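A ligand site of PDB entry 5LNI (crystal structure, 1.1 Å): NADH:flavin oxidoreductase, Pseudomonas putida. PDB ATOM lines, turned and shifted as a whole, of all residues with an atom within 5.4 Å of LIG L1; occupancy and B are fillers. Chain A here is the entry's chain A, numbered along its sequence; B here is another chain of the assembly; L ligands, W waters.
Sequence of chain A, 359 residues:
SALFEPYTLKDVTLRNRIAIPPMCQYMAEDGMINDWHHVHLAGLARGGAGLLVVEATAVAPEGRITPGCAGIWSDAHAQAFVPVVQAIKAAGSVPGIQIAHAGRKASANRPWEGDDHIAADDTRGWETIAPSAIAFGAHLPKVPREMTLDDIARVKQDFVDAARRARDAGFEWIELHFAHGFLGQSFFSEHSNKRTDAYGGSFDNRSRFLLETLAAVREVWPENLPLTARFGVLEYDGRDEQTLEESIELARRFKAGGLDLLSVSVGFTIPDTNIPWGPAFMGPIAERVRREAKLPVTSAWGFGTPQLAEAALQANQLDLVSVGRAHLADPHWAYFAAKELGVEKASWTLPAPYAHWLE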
ATOM      1  N   PRO A  21      -1.082  -7.238 -22.710  1.00  0.00           N
ATOM      2  CA  PRO A  21      -0.673  -6.541 -21.496  1.00  0.00           C
ATOM      3  C   PRO A  21       0.589  -7.193 -20.954  1.00  0.00           C
ATOM      4  O   PRO A  21       0.931  -8.328 -21.317  1.00  0.00           O
ATOM      5  CB  PRO A  21      -1.852  -6.763 -20.554  1.00  0.00           C
ATOM      6  CG  PRO A  21      -2.378  -8.094 -20.955  1.00  0.00           C
ATOM      7  CD  PRO A  21      -2.195  -8.160 -22.445  1.00  0.00           C
ATOM      8  N   PRO A  22       1.274  -6.509 -20.031  1.00  0.00           N
ATOM      9  CA  PRO A  22       2.460  -7.081 -19.412  1.00  0.00           C
ATOM     10  C   PRO A  22       2.107  -8.386 -18.724  1.00  0.00           C
ATOM     11  O   PRO A  22       1.154  -8.487 -17.975  1.00  0.00           O
ATOM     12  CB  PRO A  22       2.897  -5.999 -18.395  1.00  0.00           C
ATOM     13  CG  PRO A  22       1.636  -5.178 -18.160  1.00  0.00           C
ATOM     14  CD  PRO A  22       0.937  -5.179 -19.473  1.00  0.00           C
ATOM     15  N   MET A  23       2.943  -9.392 -18.968  1.00  0.00           N
ATOM     16  CA  MET A  23       2.804 -10.719 -18.348  1.00  0.00           C
ATOM     17  C   MET A  23       4.163 -11.273 -17.928  1.00  0.00           C
ATOM     18  O   MET A  23       4.927 -11.792 -18.763  1.00  0.00           O
ATOM     19  CB  MET A  23       2.065 -11.728 -19.220  1.00  0.00           C
ATOM     20  CG  MET A  23       0.589 -11.427 -19.342  1.00  0.00           C
ATOM     21  SD  MET A  23      -0.302 -12.633 -20.349  1.00  0.00           S
ATOM     22  CE  MET A  23       0.292 -12.164 -21.949  1.00  0.00           C
ATOM     23  N   CYS A  24       4.484 -11.148 -16.648  1.00  0.00           N
ATOM     24  CA  CYS A  24       5.679 -11.748 -16.085  1.00  0.00           C
ATOM     25  C   CYS A  24       5.869 -13.189 -16.522  1.00  0.00           C
ATOM     26  O   CYS A  24       4.937 -14.009 -16.508  1.00  0.00           O
ATOM     27  CB  CYS A  24       5.612 -11.690 -14.580  1.00  0.00           C
ATOM     28  SG  CYS A  24       5.959 -10.099 -13.823  1.00  0.00           S
ATOM     29  N   GLN A  25       7.110 -13.494 -16.868  1.00  0.00           N
ATOM     30  CA  GLN A  25       7.517 -14.819 -17.300  1.00  0.00           C
ATOM     31  C   GLN A  25       8.346 -15.568 -16.255  1.00  0.00           C
ATOM     32  O   GLN A  25       8.496 -16.799 -16.341  1.00  0.00           O
ATOM     33  CB  GLN A  25       8.296 -14.715 -18.621  1.00  0.00           C
ATOM     34  CG  GLN A  25       7.467 -14.146 -19.767  1.00  0.00           C
ATOM     35  CD  GLN A  25       6.332 -15.052 -20.130  1.00  0.00           C
ATOM     36  OE1 GLN A  25       6.531 -16.115 -20.708  1.00  0.00           O
ATOM     37  NE2 GLN A  25       5.111 -14.637 -19.760  1.00  0.00           N
ATOM     38  N   TYR A  26       8.933 -14.832 -15.309  1.00  0.00           N
ATOM     39  CA  TYR A  26       9.713 -15.445 -14.220  1.00  0.00           C
ATOM     40  C   TYR A  26      10.906 -16.239 -14.721  1.00  0.00           C
ATOM     41  O   TYR A  26      11.311 -17.212 -14.087  1.00  0.00           O
ATOM     42  CB  TYR A  26       8.807 -16.268 -13.267  1.00  0.00           C
ATOM     43  CG  TYR A  26       7.568 -15.532 -12.840  1.00  0.00           C
ATOM     44  CD1 TYR A  26       7.560 -14.715 -11.723  1.00  0.00           C
ATOM     45  CD2 TYR A  26       6.391 -15.654 -13.579  1.00  0.00           C
ATOM     46  CE1 TYR A  26       6.427 -14.020 -11.338  1.00  0.00           C
ATOM     47  CE2 TYR A  26       5.251 -14.971 -13.199  1.00  0.00           C
ATOM     48  CZ  TYR A  26       5.260 -14.176 -12.071  1.00  0.00           C
ATOM     49  OH  TYR A  26       4.104 -13.513 -11.731  1.00  0.00           O
ATOM     50  N   GLU A  55       6.482  -7.407 -19.854  1.00  0.00           N
ATOM     51  CA  GLU A  55       6.241  -7.686 -18.443  1.00  0.00           C
ATOM     52  C   GLU A  55       6.865  -6.678 -17.492  1.00  0.00           C
ATOM     53  O   GLU A  55       7.867  -6.023 -17.817  1.00  0.00           O
ATOM     54  CB  GLU A  55       6.845  -9.064 -18.087  1.00  0.00           C
ATOM     55  CG  GLU A  55       8.372  -9.170 -18.249  1.00  0.00           C
ATOM     56  CD  GLU A  55       8.819 -10.607 -18.274  1.00  0.00           C
ATOM     57  OE1 GLU A  55       8.983 -11.212 -17.185  1.00  0.00           O
ATOM     58  OE2 GLU A  55       8.939 -11.159 -19.376  1.00  0.00           O
ATOM     59  N   ALA A  56       6.288  -6.609 -16.295  1.00  0.00           N
ATOM     60  CA  ALA A  56       6.832  -5.796 -15.200  1.00  0.00           C
ATOM     61  C   ALA A  56       8.344  -5.962 -15.122  1.00  0.00           C
ATOM     62  O   ALA A  56       8.845  -7.046 -14.823  1.00  0.00           O
ATOM     63  CB  ALA A  56       6.206  -6.219 -13.884  1.00  0.00           C
ATOM     64  N   GLN A  98       6.494  -2.190 -19.333  1.00  0.00           N
ATOM     65  CA  GLN A  98       6.009  -1.788 -18.011  1.00  0.00           C
ATOM     66  C   GLN A  98       7.176  -1.743 -17.042  1.00  0.00           C
ATOM     67  O   GLN A  98       7.836  -2.763 -16.854  1.00  0.00           O
ATOM     68  CB  GLN A  98       4.940  -2.758 -17.520  1.00  0.00           C
ATOM     69  CG  GLN A  98       4.293  -2.297 -16.252  1.00  0.00           C
ATOM     70  CD  GLN A  98       3.430  -3.339 -15.631  1.00  0.00           C
ATOM     71  OE1 GLN A  98       3.909  -4.415 -15.314  1.00  0.00           O
ATOM     72  NE2 GLN A  98       2.146  -3.025 -15.450  1.00  0.00           N
ATOM     73  N   GLU A 175       4.721   2.081 -19.697  1.00  0.00           N
ATOM     74  CA  GLU A 175       3.656   1.967 -18.720  1.00  0.00           C
ATOM     75  C   GLU A 175       4.276   1.953 -17.328  1.00  0.00           C
ATOM     76  O   GLU A 175       5.074   1.069 -17.008  1.00  0.00           O
ATOM     77  CB  GLU A 175       2.841   0.697 -18.940  1.00  0.00           C
ATOM     78  CG  GLU A 175       1.653   0.583 -18.015  1.00  0.00           C
ATOM     79  CD  GLU A 175       0.873  -0.701 -18.256  1.00  0.00           C
ATOM     80  OE1 GLU A 175       0.220  -0.832 -19.313  1.00  0.00           O
ATOM     81  OE2 GLU A 175       0.902  -1.596 -17.433  1.00  0.00           O
ATOM     82  N   HIS A 177       4.004   1.072 -13.552  1.00  0.00           N
ATOM     83  CA  HIS A 177       3.208   0.085 -12.837  1.00  0.00           C
ATOM     84  C   HIS A 177       2.824   0.643 -11.470  1.00  0.00           C
ATOM     85  O   HIS A 177       3.523   0.431 -10.481  1.00  0.00           O
ATOM     86  CB  HIS A 177       3.979  -1.217 -12.687  1.00  0.00           C
ATOM     87  CG  HIS A 177       3.111  -2.348 -12.290  1.00  0.00           C
ATOM     88  ND1 HIS A 177       1.793  -2.175 -11.904  1.00  0.00           N
ATOM     89  CD2 HIS A 177       3.334  -3.691 -12.335  1.00  0.00           C
ATOM     90  CE1 HIS A 177       1.256  -3.370 -11.729  1.00  0.00           C
ATOM     91  NE2 HIS A 177       2.166  -4.309 -11.974  1.00  0.00           N
ATOM     92  N   HIS A 180      -1.816  -3.114  -8.540  1.00  0.00           N
ATOM     93  CA  HIS A 180      -1.633  -4.510  -8.087  1.00  0.00           C
ATOM     94  C   HIS A 180      -0.932  -4.629  -6.761  1.00  0.00           C
ATOM     95  O   HIS A 180      -0.323  -5.654  -6.449  1.00  0.00           O
ATOM     96  CB  HIS A 180      -0.992  -5.362  -9.185  1.00  0.00           C
ATOM     97  CG  HIS A 180      -1.782  -5.335 -10.465  1.00  0.00           C
ATOM     98  ND1 HIS A 180      -1.261  -5.723 -11.674  1.00  0.00           N
ATOM     99  CD2 HIS A 180      -3.044  -4.906 -10.731  1.00  0.00           C
ATOM    100  CE1 HIS A 180      -2.165  -5.554 -12.625  1.00  0.00           C
ATOM    101  NE2 HIS A 180      -3.260  -5.074 -12.076  1.00  0.00           N
ATOM    102  N   ARG A 230      -0.516   1.958 -15.342  1.00  0.00           N
ATOM    103  CA  ARG A 230      -1.508   1.005 -14.842  1.00  0.00           C
ATOM    104  C   ARG A 230      -1.824   1.361 -13.395  1.00  0.00           C
ATOM    105  O   ARG A 230      -0.913   1.615 -12.611  1.00  0.00           O
ATOM    106  CB  ARG A 230      -1.038  -0.439 -14.960  1.00  0.00           C
ATOM    107  CG  ARG A 230      -2.190  -1.440 -14.890  1.00  0.00           C
ATOM    108  CD  ARG A 230      -1.783  -2.839 -15.333  1.00  0.00           C
ATOM    109  NE  ARG A 230      -2.956  -3.569 -15.823  1.00  0.00           N
ATOM    110  CZ  ARG A 230      -2.927  -4.803 -16.313  1.00  0.00           C
ATOM    111  NH1 ARG A 230      -4.040  -5.305 -16.864  1.00  0.00           N
ATOM    112  NH2 ARG A 230      -1.848  -5.538 -16.259  1.00  0.00           N
ATOM    113  N   ALA A 300      -8.446  -5.264 -18.732  1.00  0.00           N
ATOM    114  CA  ALA A 300      -8.173  -6.673 -18.921  1.00  0.00           C
ATOM    115  C   ALA A 300      -9.061  -7.448 -17.937  1.00  0.00           C
ATOM    116  O   ALA A 300     -10.044  -6.920 -17.447  1.00  0.00           O
ATOM    117  CB  ALA A 300      -6.683  -6.985 -18.718  1.00  0.00           C
ATOM    118  N   TRP A 301      -8.659  -8.661 -17.595  1.00  0.00           N
ATOM    119  CA  TRP A 301      -9.310  -9.503 -16.592  1.00  0.00           C
ATOM    120  C   TRP A 301     -10.662  -9.968 -17.098  1.00  0.00           C
ATOM    121  O   TRP A 301     -11.673  -9.859 -16.392  1.00  0.00           O
ATOM    122  CB  TRP A 301      -9.440  -8.813 -15.230  1.00  0.00           C
ATOM    123  CG  TRP A 301      -8.188  -8.176 -14.713  1.00  0.00           C
ATOM    124  CD1 TRP A 301      -7.887  -6.850 -14.727  1.00  0.00           C
ATOM    125  CD2 TRP A 301      -7.062  -8.830 -14.101  1.00  0.00           C
ATOM    126  NE1 TRP A 301      -6.663  -6.633 -14.160  1.00  0.00           N
ATOM    127  CE2 TRP A 301      -6.119  -7.832 -13.785  1.00  0.00           C
ATOM    128  CE3 TRP A 301      -6.758 -10.171 -13.814  1.00  0.00           C
ATOM    129  CZ2 TRP A 301      -4.887  -8.122 -13.179  1.00  0.00           C
ATOM    130  CZ3 TRP A 301      -5.552 -10.445 -13.209  1.00  0.00           C
ATOM    131  CH2 TRP A 301      -4.625  -9.428 -12.893  1.00  0.00           C
ATOM    132  N   GLY A 302     -10.680 -10.581 -18.277  1.00  0.00           N
ATOM    133  CA  GLY A 302     -11.889 -11.183 -18.794  1.00  0.00           C
ATOM    134  C   GLY A 302     -12.397 -10.679 -20.116  1.00  0.00           C
ATOM    135  O   GLY A 302     -13.548 -10.978 -20.419  1.00  0.00           O
ATOM    136  N   PHE A 303     -11.608  -9.962 -20.916  1.00  0.00           N
ATOM    137  CA  PHE A 303     -12.062  -9.541 -22.249  1.00  0.00           C
ATOM    138  C   PHE A 303     -11.567 -10.462 -23.360  1.00  0.00           C
ATOM    139  O   PHE A 303     -11.758 -10.166 -24.537  1.00  0.00           O
ATOM    140  CB  PHE A 303     -11.623  -8.105 -22.582  1.00  0.00           C
ATOM    141  CG  PHE A 303     -12.226  -7.055 -21.687  1.00  0.00           C
ATOM    142  CD1 PHE A 303     -13.463  -6.494 -21.975  1.00  0.00           C
ATOM    143  CD2 PHE A 303     -11.521  -6.592 -20.600  1.00  0.00           C
ATOM    144  CE1 PHE A 303     -13.990  -5.523 -21.157  1.00  0.00           C
ATOM    145  CE2 PHE A 303     -12.020  -5.613 -19.781  1.00  0.00           C
ATOM    146  CZ  PHE A 303     -13.267  -5.091 -20.042  1.00  0.00           C
ATOM    147  N   GLY A 304     -10.973 -11.583 -23.000  1.00  0.00           N
ATOM    148  CA  GLY A 304     -10.301 -12.435 -23.959  1.00  0.00           C
ATOM    149  C   GLY A 304     -11.146 -13.365 -24.795  1.00  0.00           C
ATOM    150  O   GLY A 304     -10.815 -14.537 -24.942  1.00  0.00           O
ATOM    151  N   SER A 322      -7.012  -5.237 -23.745  1.00  0.00           N
ATOM    152  CA  SER A 322      -5.856  -6.027 -23.361  1.00  0.00           C
ATOM    153  C   SER A 322      -6.282  -7.470 -23.175  1.00  0.00           C
ATOM    154  O   SER A 322      -7.247  -7.746 -22.446  1.00  0.00           O
ATOM    155  CB  SER A 322      -5.241  -5.471 -22.090  1.00  0.00           C
ATOM    156  OG  SER A 322      -4.689  -4.180 -22.313  1.00  0.00           O
ATOM    157  N   VAL A 323      -5.548  -8.366 -23.832  1.00  0.00           N
ATOM    158  CA  VAL A 323      -5.872  -9.793 -23.860  1.00  0.00           C
ATOM    159  C   VAL A 323      -4.609 -10.561 -23.456  1.00  0.00           C
ATOM    160  O   VAL A 323      -3.638 -10.599 -24.192  1.00  0.00           O
ATOM    161  CB  VAL A 323      -6.387 -10.224 -25.240  1.00  0.00           C
ATOM    162  CG1 VAL A 323      -6.605 -11.737 -25.286  1.00  0.00           C
ATOM    163  CG2 VAL A 323      -7.637  -9.469 -25.607  1.00  0.00           C
ATOM    164  N   GLY A 324      -4.625 -11.119 -22.238  1.00  0.00           N
ATOM    165  CA  GLY A 324      -3.451 -11.719 -21.641  1.00  0.00           C
ATOM    166  C   GLY A 324      -3.356 -13.232 -21.789  1.00  0.00           C
ATOM    167  O   GLY A 324      -2.659 -13.734 -22.675  1.00  0.00           O
ATOM    168  N   ARG A 325      -4.081 -13.957 -20.957  1.00  0.00           N
ATOM    169  CA  ARG A 325      -3.959 -15.424 -20.923  1.00  0.00           C
ATOM    170  C   ARG A 325      -4.274 -16.088 -22.244  1.00  0.00           C
ATOM    171  O   ARG A 325      -3.693 -17.145 -22.557  1.00  0.00           O
ATOM    172  CB  ARG A 325      -4.849 -16.013 -19.825  1.00  0.00           C
ATOM    173  CG  ARG A 325      -4.301 -15.810 -18.427  1.00  0.00           C
ATOM    174  CD  ARG A 325      -5.334 -16.149 -17.366  1.00  0.00           C
ATOM    175  NE  ARG A 325      -6.487 -15.260 -17.477  1.00  0.00           N
ATOM    176  CZ  ARG A 325      -7.765 -15.634 -17.358  1.00  0.00           C
ATOM    177  NH1 ARG A 325      -8.095 -16.899 -17.128  1.00  0.00           N
ATOM    178  NH2 ARG A 325      -8.716 -14.726 -17.484  1.00  0.00           N
ATOM    179  N   ALA A 326      -5.187 -15.524 -23.020  1.00  0.00           N
ATOM    180  CA  ALA A 326      -5.491 -16.115 -24.320  1.00  0.00           C
ATOM    181  C   ALA A 326      -4.275 -16.133 -25.241  1.00  0.00           C
ATOM    182  O   ALA A 326      -4.179 -17.009 -26.109  1.00  0.00           O
ATOM    183  CB  ALA A 326      -6.650 -15.416 -24.974  1.00  0.00           C
ATOM    184  N   LEU A 328      -1.112 -16.541 -24.069  1.00  0.00           N
ATOM    185  CA  LEU A 328      -0.269 -17.624 -23.589  1.00  0.00           C
ATOM    186  C   LEU A 328      -0.748 -18.935 -24.197  1.00  0.00           C
ATOM    187  O   LEU A 328       0.041 -19.771 -24.613  1.00  0.00           O
ATOM    188  CB  LEU A 328      -0.272 -17.683 -22.066  1.00  0.00           C
ATOM    189  CG  LEU A 328       0.107 -16.386 -21.343  1.00  0.00           C
ATOM    190  CD1 LEU A 328       0.083 -16.591 -19.837  1.00  0.00           C
ATOM    191  CD2 LEU A 328       1.433 -15.812 -21.808  1.00  0.00           C
ATOM    192  N   PRO B 353       5.884 -21.144 -17.590  1.00  0.00           N
ATOM    193  CA  PRO B 353       5.410 -19.758 -17.639  1.00  0.00           C
ATOM    194  C   PRO B 353       4.097 -19.580 -18.373  1.00  0.00           C
ATOM    195  O   PRO B 353       3.504 -18.511 -18.284  1.00  0.00           O
ATOM    196  CB  PRO B 353       6.556 -19.017 -18.350  1.00  0.00           C
ATOM    197  CG  PRO B 353       7.761 -19.869 -18.141  1.00  0.00           C
ATOM    198  CD  PRO B 353       7.244 -21.275 -18.160  1.00  0.00           C
ATOM    199  N   TRP B 357      -0.698 -20.872 -15.627  1.00  0.00           N
ATOM    200  CA  TRP B 357      -1.814 -19.934 -15.699  1.00  0.00           C
ATOM    201  C   TRP B 357      -2.991 -20.498 -16.445  1.00  0.00           C
ATOM    202  O   TRP B 357      -4.060 -19.914 -16.391  1.00  0.00           O
ATOM    203  CB  TRP B 357      -1.337 -18.663 -16.383  1.00  0.00           C
ATOM    204  CG  TRP B 357      -0.109 -18.167 -15.728  1.00  0.00           C
ATOM    205  CD1 TRP B 357       1.159 -18.233 -16.226  1.00  0.00           C
ATOM    206  CD2 TRP B 357      -0.012 -17.615 -14.421  1.00  0.00           C
ATOM    207  NE1 TRP B 357       2.039 -17.759 -15.297  1.00  0.00           N
ATOM    208  CE2 TRP B 357       1.348 -17.359 -14.194  1.00  0.00           C
ATOM    209  CE3 TRP B 357      -0.937 -17.303 -13.416  1.00  0.00           C
ATOM    210  CZ2 TRP B 357       1.801 -16.777 -13.025  1.00  0.00           C
ATOM    211  CZ3 TRP B 357      -0.479 -16.739 -12.256  1.00  0.00           C
ATOM    212  CH2 TRP B 357       0.898 -16.470 -12.069  1.00  0.00           C
HETATM  213  N1  LIG L   1      -0.037  -7.383 -14.866  1.00  0.00           N
HETATM  214  C1  LIG L   1       0.849  -6.397 -14.823  1.00  0.00           C
HETATM  215  O1  LIG L   1       0.456  -5.192 -14.687  1.00  0.00           O
HETATM  216  N2  LIG L   1       2.217  -6.680 -14.900  1.00  0.00           N
HETATM  217  C2  LIG L   1       2.713  -7.882 -15.103  1.00  0.00           C
HETATM  218  O2  LIG L   1       3.907  -8.057 -15.343  1.00  0.00           O
HETATM  219  C3  LIG L   1       1.767  -8.987 -15.026  1.00  0.00           C
HETATM  220  N3  LIG L   1       2.235 -10.277 -15.109  1.00  0.00           N
HETATM  221  C4  LIG L   1       1.309 -11.262 -15.323  1.00  0.00           C
HETATM  222  C5  LIG L   1       1.759 -12.596 -15.611  1.00  0.00           C
HETATM  223  C6  LIG L   1       0.884 -13.574 -16.003  1.00  0.00           C
HETATM  224  C7  LIG L   1       1.410 -14.880 -16.474  1.00  0.00           C
HETATM  225  C8  LIG L   1      -0.509 -13.279 -16.016  1.00  0.00           C
HETATM  226  C9  LIG L   1      -1.514 -14.349 -16.411  1.00  0.00           C
HETATM  227  C10 LIG L   1      -0.975 -12.002 -15.664  1.00  0.00           C
HETATM  228  C11 LIG L   1      -0.058 -10.947 -15.386  1.00  0.00           C
HETATM  229  N4  LIG L   1      -0.508  -9.648 -15.168  1.00  0.00           N
HETATM  230  C12 LIG L   1       0.410  -8.634 -14.996  1.00  0.00           C
HETATM  231  C13 LIG L   1      -1.929  -9.321 -15.384  1.00  0.00           C
HETATM  232  C14 LIG L   1      -2.241  -9.327 -16.888  1.00  0.00           C
HETATM  233  O3  LIG L   1      -1.656  -8.183 -17.531  1.00  0.00           O
HETATM  234  C15 LIG L   1      -3.749  -9.279 -17.172  1.00  0.00           C
HETATM  235  O4  LIG L   1      -4.328  -8.161 -16.503  1.00  0.00           O
HETATM  236  C16 LIG L   1      -4.437 -10.568 -16.745  1.00  0.00           C
HETATM  237  O5  LIG L   1      -3.832 -11.669 -17.410  1.00  0.00           O
HETATM  238  C17 LIG L   1      -5.943 -10.491 -17.017  1.00  0.00           C
HETATM  239  O6  LIG L   1      -6.241 -10.438 -18.420  1.00  0.00           O
HETATM  240  P1  LIG L   1      -6.761 -11.785 -19.170  1.00  0.00           P
HETATM  241  O7  LIG L   1      -5.706 -12.844 -18.903  1.00  0.00           O
HETATM  242  O8  LIG L   1      -8.088 -12.139 -18.542  1.00  0.00           O
HETATM  243  O9  LIG L   1      -6.866 -11.386 -20.608  1.00  0.00           O
HETATM  244  O1  LG2 L   2      -2.635 -12.624 -12.544  1.00  0.00           O
HETATM  245  C1  LG2 L   2      -1.474 -12.212 -12.379  1.00  0.00           C
HETATM  246  C2  LG2 L   2      -0.319 -12.992 -12.353  1.00  0.00           C
HETATM  247  C3  LG2 L   2       0.912 -12.387 -12.167  1.00  0.00           C
HETATM  248  C4  LG2 L   2       1.034 -11.017 -11.997  1.00  0.00           C
HETATM  249  O2  LG2 L   2      -1.358 -10.857 -12.204  1.00  0.00           O
HETATM  250  C5  LG2 L   2      -0.136 -10.260 -12.031  1.00  0.00           C
HETATM  251  C6  LG2 L   2      -0.144  -8.867 -11.913  1.00  0.00           C
HETATM  252  C7  LG2 L   2       1.080  -8.202 -11.787  1.00  0.00           C
HETATM  253  O3  LG2 L   2       1.099  -6.903 -11.768  1.00  0.00           O
HETATM  254  C8  LG2 L   2       2.267  -8.949 -11.739  1.00  0.00           C
HETATM  255  C9  LG2 L   2       2.230 -10.325 -11.845  1.00  0.00           C
HETATM  256  O   HOH W   1      -8.799  -9.497 -20.934  1.00  0.00           O
HETATM  257  O   HOH W   2      -7.210 -13.670 -22.241  1.00  0.00           O
HETATM  258  O   HOH W   3      -9.895 -12.839 -20.614  1.00  0.00           O
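N of Trp 301 is in hydrogen-bond range of O6 of LIG L1, at 3.1 Å.
O8 of LIG L1 lies within salt-bridge range of NH2 of Arg 325 (2.9 Å).
An oxygen (O3) of LG2 L2 is in hydrogen-bond range of a ring nitrogen (ND1) of His 180 (2.6 Å).
An oxygen (O1) of LIG L1 lies within hydrogen-bond range of a ring nitrogen (NE2) of His 177 (3.3 Å).
The side-chain sulfur of Cys 24 sits at hydrogen-bond distance from an oxygen (O2) of LIG L1 (3.3 Å).
An oxygen (O7) of LIG L1 lies within hydrogen-bond range of the backbone NH (N) of Arg 325 (2.8 Å).
N of Cys 24 sits at hydrogen-bond distance from N3 of LIG L1 (2.9 Å).
NH2 of Arg 230 is in hydrogen-bond range of O1 of LIG L1, 2.8 Å away.
NE2 of Gln 98 is in hydrogen-bond range of O1 of LIG L1, at 2.9 Å.
A ring nitrogen (NE2) of His 177 sits at hydrogen-bond distance from an oxygen (O3) of LG2 L2 (2.8 Å).
O8 of LIG L1 sits at hydrogen-bond distance from N of Gly 302, at 3.0 Å.
The backbone NH (N) of Ala 56 lies within hydrogen-bond range of an oxygen (O2) of LIG L1 (2.9 Å).
An oxygen (O3) of LIG L1 is in hydrogen-bond range of the backbone carbonyl oxygen (O) of Pro 22, 2.9 Å away.
The backbone NH (N) of Gly 324 lies within hydrogen-bond range of an oxygen (O9) of LIG L1 (2.8 Å).
N2 of LIG L1 lies close to O3 of LG2 L2 (3.3 Å).
The side-chain amide oxygen (OE1) of Gln 98 sits close to the backbone NH (N) of Ala 56.
NE2 of Gln 25 is in hydrogen-bond range of O of Met 23, at 3.0 Å.
The side-chain carboxylate (OE1) of Glu 55 sits at hydrogen-bond distance from the backbone NH (N) of Gln 25, 3.0 Å away.
The indole nitrogen (NE1) of Trp 357 of chain B sits close to the backbone carbonyl oxygen (O) of Pro 353 of chain B (3.4 Å).
The side-chain amide nitrogen of Gln 98 is in hydrogen-bond range of the side-chain carboxylate of Glu 175.
Pro 21 touches LIG L1 (CB to O3, 3.3 Å).
Met 23 touches LIG L1.
Glu 55 touches LIG L1.
His 180 touches LIG L1.
Ala 300 touches LIG L1.
Val 323 touches LIG L1 (C to O9, 3.7 Å).
Leu 328 touches LIG L1 (CD1 to C7, 3.9998 Å).
Trp 357 of chain B touches LIG L1 (NE1 to C7, 3.2 Å).
The nearest printed residue that does not touch LIG L1 is Ser 322 (4.1 Å).
Water W2 lies within hydrogen-bond range of an oxygen (O9) of LIG L1, the backbone NH (N) of Ala 326 and the backbone NH (N) of Arg 325.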
